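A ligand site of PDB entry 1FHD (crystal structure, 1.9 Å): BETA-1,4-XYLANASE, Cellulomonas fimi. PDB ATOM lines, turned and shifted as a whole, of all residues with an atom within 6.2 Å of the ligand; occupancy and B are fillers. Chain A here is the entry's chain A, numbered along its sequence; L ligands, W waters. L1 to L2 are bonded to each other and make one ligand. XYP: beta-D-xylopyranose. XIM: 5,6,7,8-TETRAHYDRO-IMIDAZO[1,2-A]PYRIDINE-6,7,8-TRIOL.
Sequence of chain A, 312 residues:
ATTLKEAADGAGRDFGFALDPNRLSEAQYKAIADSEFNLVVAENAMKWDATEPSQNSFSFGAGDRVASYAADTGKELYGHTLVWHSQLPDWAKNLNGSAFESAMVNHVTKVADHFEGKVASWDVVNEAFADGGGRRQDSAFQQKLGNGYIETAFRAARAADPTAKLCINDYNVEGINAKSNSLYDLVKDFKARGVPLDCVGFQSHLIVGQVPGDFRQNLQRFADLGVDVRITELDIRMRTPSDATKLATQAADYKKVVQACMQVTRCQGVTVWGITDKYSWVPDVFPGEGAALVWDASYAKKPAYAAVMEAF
The side-chain carboxylate (OE2) of Glu 127 lies within hydrogen-bond range of a nitrogen (N21) of XIM L2, at 2.5 Å.
The side-chain carboxylate (OE2) of Glu 43 lies within hydrogen-bond range of an oxygen (O2) of XYP L1 (2.6 Å).
The side-chain carboxylate (OE2) of Glu 233 lies within hydrogen-bond range of an oxygen (O2) of XIM L2 (2.6 Å).
NE1 of Trp 273 is in hydrogen-bond range of O2 of XYP L1, 2.8 Å away.
An oxygen (O3) of XIM L2 is in hydrogen-bond range of the side-chain amino group (NZ) of Lys 47 (2.8 Å).
NE2 of His 80 lies within hydrogen-bond range of O3 of XIM L2.
N21 of XIM L2 lies close to OE1 of Gln 203.
The side-chain amide oxygen (OD1) of Asn 44 sits at hydrogen-bond distance from an oxygen (O3) of XYP L1, at 3.1 Å.
The side-chain amide nitrogen (ND2) of Asn 126 is in hydrogen-bond range of an oxygen (O2) of XIM L2 (3.1 Å).
The side-chain amide nitrogen (NE2) of Gln 87 is in hydrogen-bond range of an oxygen (O5) of XYP L1 (3.2 Å).
OE2 of Glu 127 lies within hydrogen-bond range of ND2 of Asn 126 (3.5 Å).
The side-chain carboxylate of Glu 127 sits at hydrogen-bond distance from the indole nitrogen of Trp 84 (3.0 Å).
NZ of Lys 47 sits close to ND2 of Asn 44, 2.7 Å away.
The side-chain amino group (NZ) of Lys 47 sits close to the side-chain amide nitrogen (NE2) of Gln 87 (3.0 Å).
NE2 of Gln 203 sits close to ND2 of Asn 169, 3.2 Å away.
OE1 of Gln 87 is in hydrogen-bond range of ND2 of Asn 44 (3.1 Å).
The side-chain amide nitrogen (ND2) of Asn 126 lies close to the indole nitrogen (NE1) of Trp 84 (3.2 Å).
The backbone carbonyl oxygen (O) of Trp 281 lies close to the side-chain carboxylate (OD2) of Asp 284, 2.6 Å away.
Trp 84 touches the ligand.
His 205 touches the ligand.
Trp 281 touches the ligand.
Of the 20 residues printed, 13 come within 4 Å of the ligand.
The nearest printed residue that does not touch the ligand is Tyr 171 (4.2 Å).
Water W2 lies within hydrogen-bond range of O of Tyr 279 (2.8 Å), OE2 of Glu 43 (2.9 Å) and O3 of XYP L1 (3.4 Å).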
ATOM      1  N   GLU A  43      27.289  -4.265   9.923  1.00  0.00           N
ATOM      2  CA  GLU A  43      26.931  -5.332  10.861  1.00  0.00           C
ATOM      3  C   GLU A  43      25.592  -5.966  10.475  1.00  0.00           C
ATOM      4  O   GLU A  43      25.381  -7.160  10.678  1.00  0.00           O
ATOM      5  CB  GLU A  43      26.858  -4.787  12.282  1.00  0.00           C
ATOM      6  CG  GLU A  43      26.447  -5.825  13.298  1.00  0.00           C
ATOM      7  CD  GLU A  43      26.339  -5.269  14.711  1.00  0.00           C
ATOM      8  OE1 GLU A  43      26.031  -4.063  14.849  1.00  0.00           O
ATOM      9  OE2 GLU A  43      26.551  -6.053  15.658  1.00  0.00           O
ATOM     10  N   ASN A  44      24.687  -5.158   9.917  1.00  0.00           N
ATOM     11  CA  ASN A  44      23.366  -5.639   9.514  1.00  0.00           C
ATOM     12  C   ASN A  44      22.767  -4.998   8.262  1.00  0.00           C
ATOM     13  O   ASN A  44      21.959  -5.617   7.586  1.00  0.00           O
ATOM     14  CB  ASN A  44      22.349  -5.447  10.649  1.00  0.00           C
ATOM     15  CG  ASN A  44      22.625  -6.335  11.845  1.00  0.00           C
ATOM     16  OD1 ASN A  44      23.055  -5.866  12.893  1.00  0.00           O
ATOM     17  ND2 ASN A  44      22.384  -7.629  11.692  1.00  0.00           N
ATOM     18  N   LYS A  47      22.520  -6.992   4.829  1.00  0.00           N
ATOM     19  CA  LYS A  47      21.969  -8.335   4.860  1.00  0.00           C
ATOM     20  C   LYS A  47      20.684  -8.345   4.044  1.00  0.00           C
ATOM     21  O   LYS A  47      20.123  -7.297   3.726  1.00  0.00           O
ATOM     22  CB  LYS A  47      21.705  -8.778   6.299  1.00  0.00           C
ATOM     23  CG  LYS A  47      22.994  -9.032   7.080  1.00  0.00           C
ATOM     24  CD  LYS A  47      22.741  -9.321   8.551  1.00  0.00           C
ATOM     25  CE  LYS A  47      24.073  -9.555   9.265  1.00  0.00           C
ATOM     26  NZ  LYS A  47      23.928  -9.673  10.745  1.00  0.00           N
ATOM     27  N   HIS A  80      28.743  -7.559   3.399  1.00  0.00           N
ATOM     28  CA  HIS A  80      28.204  -8.658   4.201  1.00  0.00           C
ATOM     29  C   HIS A  80      26.693  -8.486   4.331  1.00  0.00           C
ATOM     30  O   HIS A  80      26.247  -7.453   4.840  1.00  0.00           O
ATOM     31  CB  HIS A  80      28.855  -8.602   5.589  1.00  0.00           C
ATOM     32  CG  HIS A  80      28.397  -9.669   6.541  1.00  0.00           C
ATOM     33  ND1 HIS A  80      28.936 -10.929   6.548  1.00  0.00           N
ATOM     34  CD2 HIS A  80      27.473  -9.647   7.523  1.00  0.00           C
ATOM     35  CE1 HIS A  80      28.376 -11.644   7.498  1.00  0.00           C
ATOM     36  NE2 HIS A  80      27.485 -10.882   8.111  1.00  0.00           N
ATOM     37  N   THR A  81      25.883  -9.432   3.842  1.00  0.00           N
ATOM     38  CA  THR A  81      26.304 -10.664   3.167  1.00  0.00           C
ATOM     39  C   THR A  81      25.165 -11.011   2.206  1.00  0.00           C
ATOM     40  O   THR A  81      23.997 -10.869   2.558  1.00  0.00           O
ATOM     41  CB  THR A  81      26.537 -11.850   4.186  1.00  0.00           C
ATOM     42  OG1 THR A  81      26.863 -13.051   3.471  1.00  0.00           O
ATOM     43  CG2 THR A  81      25.303 -12.078   5.053  1.00  0.00           C
ATOM     44  N   TRP A  84      22.733 -15.928   2.954  1.00  0.00           N
ATOM     45  CA  TRP A  84      22.876 -16.447   4.311  1.00  0.00           C
ATOM     46  C   TRP A  84      21.541 -17.026   4.776  1.00  0.00           C
ATOM     47  O   TRP A  84      20.485 -16.476   4.487  1.00  0.00           O
ATOM     48  CB  TRP A  84      23.324 -15.296   5.221  1.00  0.00           C
ATOM     49  CG  TRP A  84      23.639 -15.706   6.617  1.00  0.00           C
ATOM     50  CD1 TRP A  84      24.142 -16.896   7.036  1.00  0.00           C
ATOM     51  CD2 TRP A  84      23.522 -14.887   7.785  1.00  0.00           C
ATOM     52  NE1 TRP A  84      24.360 -16.882   8.391  1.00  0.00           N
ATOM     53  CE2 TRP A  84      23.981 -15.652   8.883  1.00  0.00           C
ATOM     54  CE3 TRP A  84      23.069 -13.581   8.023  1.00  0.00           C
ATOM     55  CZ2 TRP A  84      24.005 -15.165  10.195  1.00  0.00           C
ATOM     56  CZ3 TRP A  84      23.101 -13.085   9.328  1.00  0.00           C
ATOM     57  CH2 TRP A  84      23.563 -13.877  10.392  1.00  0.00           C
ATOM     58  N   GLN A  87      18.441 -14.257   9.039  1.00  0.00           N
ATOM     59  CA  GLN A  87      17.941 -12.928   8.695  1.00  0.00           C
ATOM     60  C   GLN A  87      17.478 -12.898   7.249  1.00  0.00           C
ATOM     61  O   GLN A  87      17.778 -11.969   6.492  1.00  0.00           O
ATOM     62  CB  GLN A  87      18.994 -11.853   8.962  1.00  0.00           C
ATOM     63  CG  GLN A  87      19.150 -11.560  10.450  1.00  0.00           C
ATOM     64  CD  GLN A  87      20.240 -10.558  10.759  1.00  0.00           C
ATOM     65  OE1 GLN A  87      20.084  -9.349  10.545  1.00  0.00           O
ATOM     66  NE2 GLN A  87      21.362 -11.059  11.261  1.00  0.00           N
ATOM     67  N   ASP A 123      30.973 -11.116   1.096  1.00  0.00           N
ATOM     68  CA  ASP A 123      30.764 -12.412   1.737  1.00  0.00           C
ATOM     69  C   ASP A 123      29.595 -12.900   0.870  1.00  0.00           C
ATOM     70  O   ASP A 123      28.431 -12.695   1.210  1.00  0.00           O
ATOM     71  CB  ASP A 123      30.283 -12.271   3.184  1.00  0.00           C
ATOM     72  CG  ASP A 123      31.425 -12.228   4.168  1.00  0.00           C
ATOM     73  OD1 ASP A 123      32.548 -12.628   3.792  1.00  0.00           O
ATOM     74  OD2 ASP A 123      31.192 -11.809   5.325  1.00  0.00           O
ATOM     75  N   ASN A 126      27.524 -17.109   3.251  1.00  0.00           N
ATOM     76  CA  ASN A 126      27.885 -17.140   4.665  1.00  0.00           C
ATOM     77  C   ASN A 126      27.359 -18.405   5.332  1.00  0.00           C
ATOM     78  O   ASN A 126      26.210 -18.796   5.117  1.00  0.00           O
ATOM     79  CB  ASN A 126      27.310 -15.886   5.354  1.00  0.00           C
ATOM     80  CG  ASN A 126      27.895 -15.645   6.729  1.00  0.00           C
ATOM     81  OD1 ASN A 126      29.082 -15.834   6.966  1.00  0.00           O
ATOM     82  ND2 ASN A 126      27.046 -15.207   7.656  1.00  0.00           N
ATOM     83  N   GLU A 127      28.230 -19.049   6.100  1.00  0.00           N
ATOM     84  CA  GLU A 127      27.896 -20.249   6.871  1.00  0.00           C
ATOM     85  C   GLU A 127      27.188 -21.373   6.115  1.00  0.00           C
ATOM     86  O   GLU A 127      26.105 -21.805   6.509  1.00  0.00           O
ATOM     87  CB  GLU A 127      27.086 -19.808   8.089  1.00  0.00           C
ATOM     88  CG  GLU A 127      27.892 -18.866   9.011  1.00  0.00           C
ATOM     89  CD  GLU A 127      27.052 -18.109  10.032  1.00  0.00           C
ATOM     90  OE1 GLU A 127      25.920 -18.530  10.327  1.00  0.00           O
ATOM     91  OE2 GLU A 127      27.553 -17.086  10.545  1.00  0.00           O
ATOM     92  N   ASN A 169      32.385 -17.112   3.736  1.00  0.00           N
ATOM     93  CA  ASN A 169      32.639 -16.853   5.160  1.00  0.00           C
ATOM     94  C   ASN A 169      32.026 -17.912   6.075  1.00  0.00           C
ATOM     95  O   ASN A 169      30.974 -18.463   5.771  1.00  0.00           O
ATOM     96  CB  ASN A 169      32.074 -15.464   5.496  1.00  0.00           C
ATOM     97  CG  ASN A 169      32.529 -14.926   6.837  1.00  0.00           C
ATOM     98  OD1 ASN A 169      33.723 -14.846   7.115  1.00  0.00           O
ATOM     99  ND2 ASN A 169      31.571 -14.526   7.660  1.00  0.00           N
ATOM    100  N   TYR A 171      32.238 -19.864  10.480  1.00  0.00           N
ATOM    101  CA  TYR A 171      32.751 -19.891  11.842  1.00  0.00           C
ATOM    102  C   TYR A 171      33.050 -21.334  12.262  1.00  0.00           C
ATOM    103  O   TYR A 171      32.566 -22.285  11.637  1.00  0.00           O
ATOM    104  CB  TYR A 171      31.733 -19.256  12.798  1.00  0.00           C
ATOM    105  CG  TYR A 171      30.446 -20.026  12.948  1.00  0.00           C
ATOM    106  CD1 TYR A 171      30.356 -21.132  13.794  1.00  0.00           C
ATOM    107  CD2 TYR A 171      29.298 -19.621  12.260  1.00  0.00           C
ATOM    108  CE1 TYR A 171      29.168 -21.838  13.943  1.00  0.00           C
ATOM    109  CE2 TYR A 171      28.088 -20.323  12.401  1.00  0.00           C
ATOM    110  CZ  TYR A 171      28.038 -21.422  13.245  1.00  0.00           C
ATOM    111  OH  TYR A 171      26.849 -22.119  13.389  1.00  0.00           O
ATOM    112  N   GLN A 203      35.421 -16.072  10.648  1.00  0.00           N
ATOM    113  CA  GLN A 203      34.748 -15.208  11.617  1.00  0.00           C
ATOM    114  C   GLN A 203      35.482 -14.995  12.924  1.00  0.00           C
ATOM    115  O   GLN A 203      35.645 -13.856  13.365  1.00  0.00           O
ATOM    116  CB  GLN A 203      33.346 -15.760  11.887  1.00  0.00           C
ATOM    117  CG  GLN A 203      32.425 -15.607  10.686  1.00  0.00           C
ATOM    118  CD  GLN A 203      31.045 -16.140  10.964  1.00  0.00           C
ATOM    119  OE1 GLN A 203      30.633 -16.250  12.123  1.00  0.00           O
ATOM    120  NE2 GLN A 203      30.313 -16.469   9.904  1.00  0.00           N
ATOM    121  N   HIS A 205      34.633 -16.017  16.153  1.00  0.00           N
ATOM    122  CA  HIS A 205      33.809 -15.645  17.306  1.00  0.00           C
ATOM    123  C   HIS A 205      34.295 -16.651  18.340  1.00  0.00           C
ATOM    124  O   HIS A 205      33.748 -17.751  18.472  1.00  0.00           O
ATOM    125  CB  HIS A 205      32.321 -15.817  17.000  1.00  0.00           C
ATOM    126  CG  HIS A 205      31.755 -14.726  16.149  1.00  0.00           C
ATOM    127  ND1 HIS A 205      31.677 -13.413  16.580  1.00  0.00           N
ATOM    128  CD2 HIS A 205      31.262 -14.724  14.888  1.00  0.00           C
ATOM    129  CE1 HIS A 205      31.164 -12.668  15.623  1.00  0.00           C
ATOM    130  NE2 HIS A 205      30.899 -13.441  14.582  1.00  0.00           N
ATOM    131  N   GLU A 233      35.014 -11.520  11.737  1.00  0.00           N
ATOM    132  CA  GLU A 233      34.106 -11.134  12.811  1.00  0.00           C
ATOM    133  C   GLU A 233      34.680 -11.409  14.197  1.00  0.00           C
ATOM    134  O   GLU A 233      33.988 -11.907  15.088  1.00  0.00           O
ATOM    135  CB  GLU A 233      32.790 -11.875  12.638  1.00  0.00           C
ATOM    136  CG  GLU A 233      32.176 -11.727  11.236  1.00  0.00           C
ATOM    137  CD  GLU A 233      30.899 -12.529  11.040  1.00  0.00           C
ATOM    138  OE1 GLU A 233      30.275 -12.920  12.054  1.00  0.00           O
ATOM    139  OE2 GLU A 233      30.516 -12.767   9.869  1.00  0.00           O
ATOM    140  N   TRP A 273      34.054  -7.617  15.317  1.00  0.00           N
ATOM    141  CA  TRP A 273      32.609  -7.478  15.193  1.00  0.00           C
ATOM    142  C   TRP A 273      31.987  -6.445  16.117  1.00  0.00           C
ATOM    143  O   TRP A 273      31.124  -6.764  16.954  1.00  0.00           O
ATOM    144  CB  TRP A 273      31.939  -8.840  15.391  1.00  0.00           C
ATOM    145  CG  TRP A 273      30.638  -8.918  14.651  1.00  0.00           C
ATOM    146  CD1 TRP A 273      29.391  -9.076  15.183  1.00  0.00           C
ATOM    147  CD2 TRP A 273      30.459  -8.783  13.241  1.00  0.00           C
ATOM    148  NE1 TRP A 273      28.449  -9.040  14.189  1.00  0.00           N
ATOM    149  CE2 TRP A 273      29.082  -8.855  12.981  1.00  0.00           C
ATOM    150  CE3 TRP A 273      31.345  -8.601  12.159  1.00  0.00           C
ATOM    151  CZ2 TRP A 273      28.545  -8.761  11.694  1.00  0.00           C
ATOM    152  CZ3 TRP A 273      30.818  -8.493  10.874  1.00  0.00           C
ATOM    153  CH2 TRP A 273      29.433  -8.579  10.658  1.00  0.00           C
ATOM    154  N   TYR A 279      27.434  -2.422  22.888  1.00  0.00           N
ATOM    155  CA  TYR A 279      26.548  -2.733  21.764  1.00  0.00           C
ATOM    156  C   TYR A 279      26.781  -4.109  21.166  1.00  0.00           C
ATOM    157  O   TYR A 279      26.060  -4.523  20.277  1.00  0.00           O
ATOM    158  CB  TYR A 279      26.674  -1.666  20.663  1.00  0.00           C
ATOM    159  CG  TYR A 279      26.162  -0.296  21.077  1.00  0.00           C
ATOM    160  CD1 TYR A 279      26.845   0.861  20.731  1.00  0.00           C
ATOM    161  CD2 TYR A 279      25.007  -0.176  21.844  1.00  0.00           C
ATOM    162  CE1 TYR A 279      26.388   2.121  21.132  1.00  0.00           C
ATOM    163  CE2 TYR A 279      24.543   1.067  22.256  1.00  0.00           C
ATOM    164  CZ  TYR A 279      25.234   2.211  21.903  1.00  0.00           C
ATOM    165  OH  TYR A 279      24.792   3.446  22.315  1.00  0.00           O
ATOM    166  N   SER A 280      27.782  -4.810  21.677  1.00  0.00           N
ATOM    167  CA  SER A 280      28.116  -6.158  21.191  1.00  0.00           C
ATOM    168  C   SER A 280      26.898  -7.077  21.147  1.00  0.00           C
ATOM    169  O   SER A 280      26.055  -7.055  22.051  1.00  0.00           O
ATOM    170  CB  SER A 280      29.187  -6.783  22.085  1.00  0.00           C
ATOM    171  OG  SER A 280      29.457  -8.126  21.704  1.00  0.00           O
ATOM    172  N   TRP A 281      26.811  -7.894  20.108  1.00  0.00           N
ATOM    173  CA  TRP A 281      25.710  -8.851  19.918  1.00  0.00           C
ATOM    174  C   TRP A 281      25.775 -10.033  20.894  1.00  0.00           C
ATOM    175  O   TRP A 281      24.782 -10.746  21.068  1.00  0.00           O
ATOM    176  CB  TRP A 281      25.759  -9.438  18.513  1.00  0.00           C
ATOM    177  CG  TRP A 281      26.910 -10.418  18.347  1.00  0.00           C
ATOM    178  CD1 TRP A 281      28.240 -10.133  18.366  1.00  0.00           C
ATOM    179  CD2 TRP A 281      26.806 -11.848  18.210  1.00  0.00           C
ATOM    180  NE1 TRP A 281      28.980 -11.289  18.256  1.00  0.00           N
ATOM    181  CE2 TRP A 281      28.118 -12.358  18.159  1.00  0.00           C
ATOM    182  CE3 TRP A 281      25.722 -12.746  18.134  1.00  0.00           C
ATOM    183  CZ2 TRP A 281      28.391 -13.727  18.046  1.00  0.00           C
ATOM    184  CZ3 TRP A 281      25.993 -14.106  18.017  1.00  0.00           C
ATOM    185  CH2 TRP A 281      27.315 -14.579  17.967  1.00  0.00           C
ATOM    186  N   ASP A 284      23.098 -10.637  24.211  1.00  0.00           N
ATOM    187  CA  ASP A 284      21.745 -10.986  23.792  1.00  0.00           C
ATOM    188  C   ASP A 284      21.606 -12.419  23.269  1.00  0.00           C
ATOM    189  O   ASP A 284      20.490 -12.938  23.149  1.00  0.00           O
ATOM    190  CB  ASP A 284      21.240  -9.999  22.726  1.00  0.00           C
ATOM    191  CG  ASP A 284      22.352  -9.451  21.822  1.00  0.00           C
ATOM    192  OD1 ASP A 284      23.198  -8.669  22.332  1.00  0.00           O
ATOM    193  OD2 ASP A 284      22.386  -9.783  20.598  1.00  0.00           O
HETATM  194  C1  XYP L   1      24.882 -10.385  14.094  1.00  0.00           C
HETATM  195  C2  XYP L   1      24.735  -8.923  14.532  1.00  0.00           C
HETATM  196  C3  XYP L   1      23.465  -8.737  15.384  1.00  0.00           C
HETATM  197  C4  XYP L   1      22.243  -9.366  14.711  1.00  0.00           C
HETATM  198  C5  XYP L   1      22.536 -10.806  14.283  1.00  0.00           C
HETATM  199  O2  XYP L   1      25.878  -8.554  15.283  1.00  0.00           O
HETATM  200  O3  XYP L   1      23.233  -7.356  15.573  1.00  0.00           O
HETATM  201  O4  XYP L   1      21.122  -9.332  15.585  1.00  0.00           O
HETATM  202  O5  XYP L   1      23.691 -10.828  13.418  1.00  0.00           O
HETATM  203  C1  XIM L   2      27.469 -14.356  12.516  1.00  0.00           C
HETATM  204  C2  XIM L   2      27.116 -13.535  11.213  1.00  0.00           C
HETATM  205  C3  XIM L   2      26.939 -12.044  11.584  1.00  0.00           C
HETATM  206  C4  XIM L   2      26.249 -11.879  12.954  1.00  0.00           C
HETATM  207  C5  XIM L   2      27.146 -12.400  14.103  1.00  0.00           C
HETATM  208  N1  XIM L   2      27.452 -13.754  13.777  1.00  0.00           N
HETATM  209  C17 XIM L   2      27.807 -14.804  14.588  1.00  0.00           C
HETATM  210  C18 XIM L   2      28.000 -15.923  13.863  1.00  0.00           C
HETATM  211  N21 XIM L   2      27.796 -15.654  12.574  1.00  0.00           N
HETATM  212  O2  XIM L   2      28.047 -13.633  10.165  1.00  0.00           O
HETATM  213  O3  XIM L   2      26.163 -11.412  10.590  1.00  0.00           O
HETATM  214  O4  XIM L   2      26.000 -10.512  13.190  1.00  0.00           O
HETATM  215  O   HOH W   1      18.665 -10.676  14.020  1.00  0.00           O
HETATM  216  O   HOH W   2      24.859  -5.605  17.972  1.00  0.00           O
HETATM  217  O   HOH W   3      22.328  -6.882  18.445  1.00  0.00           O
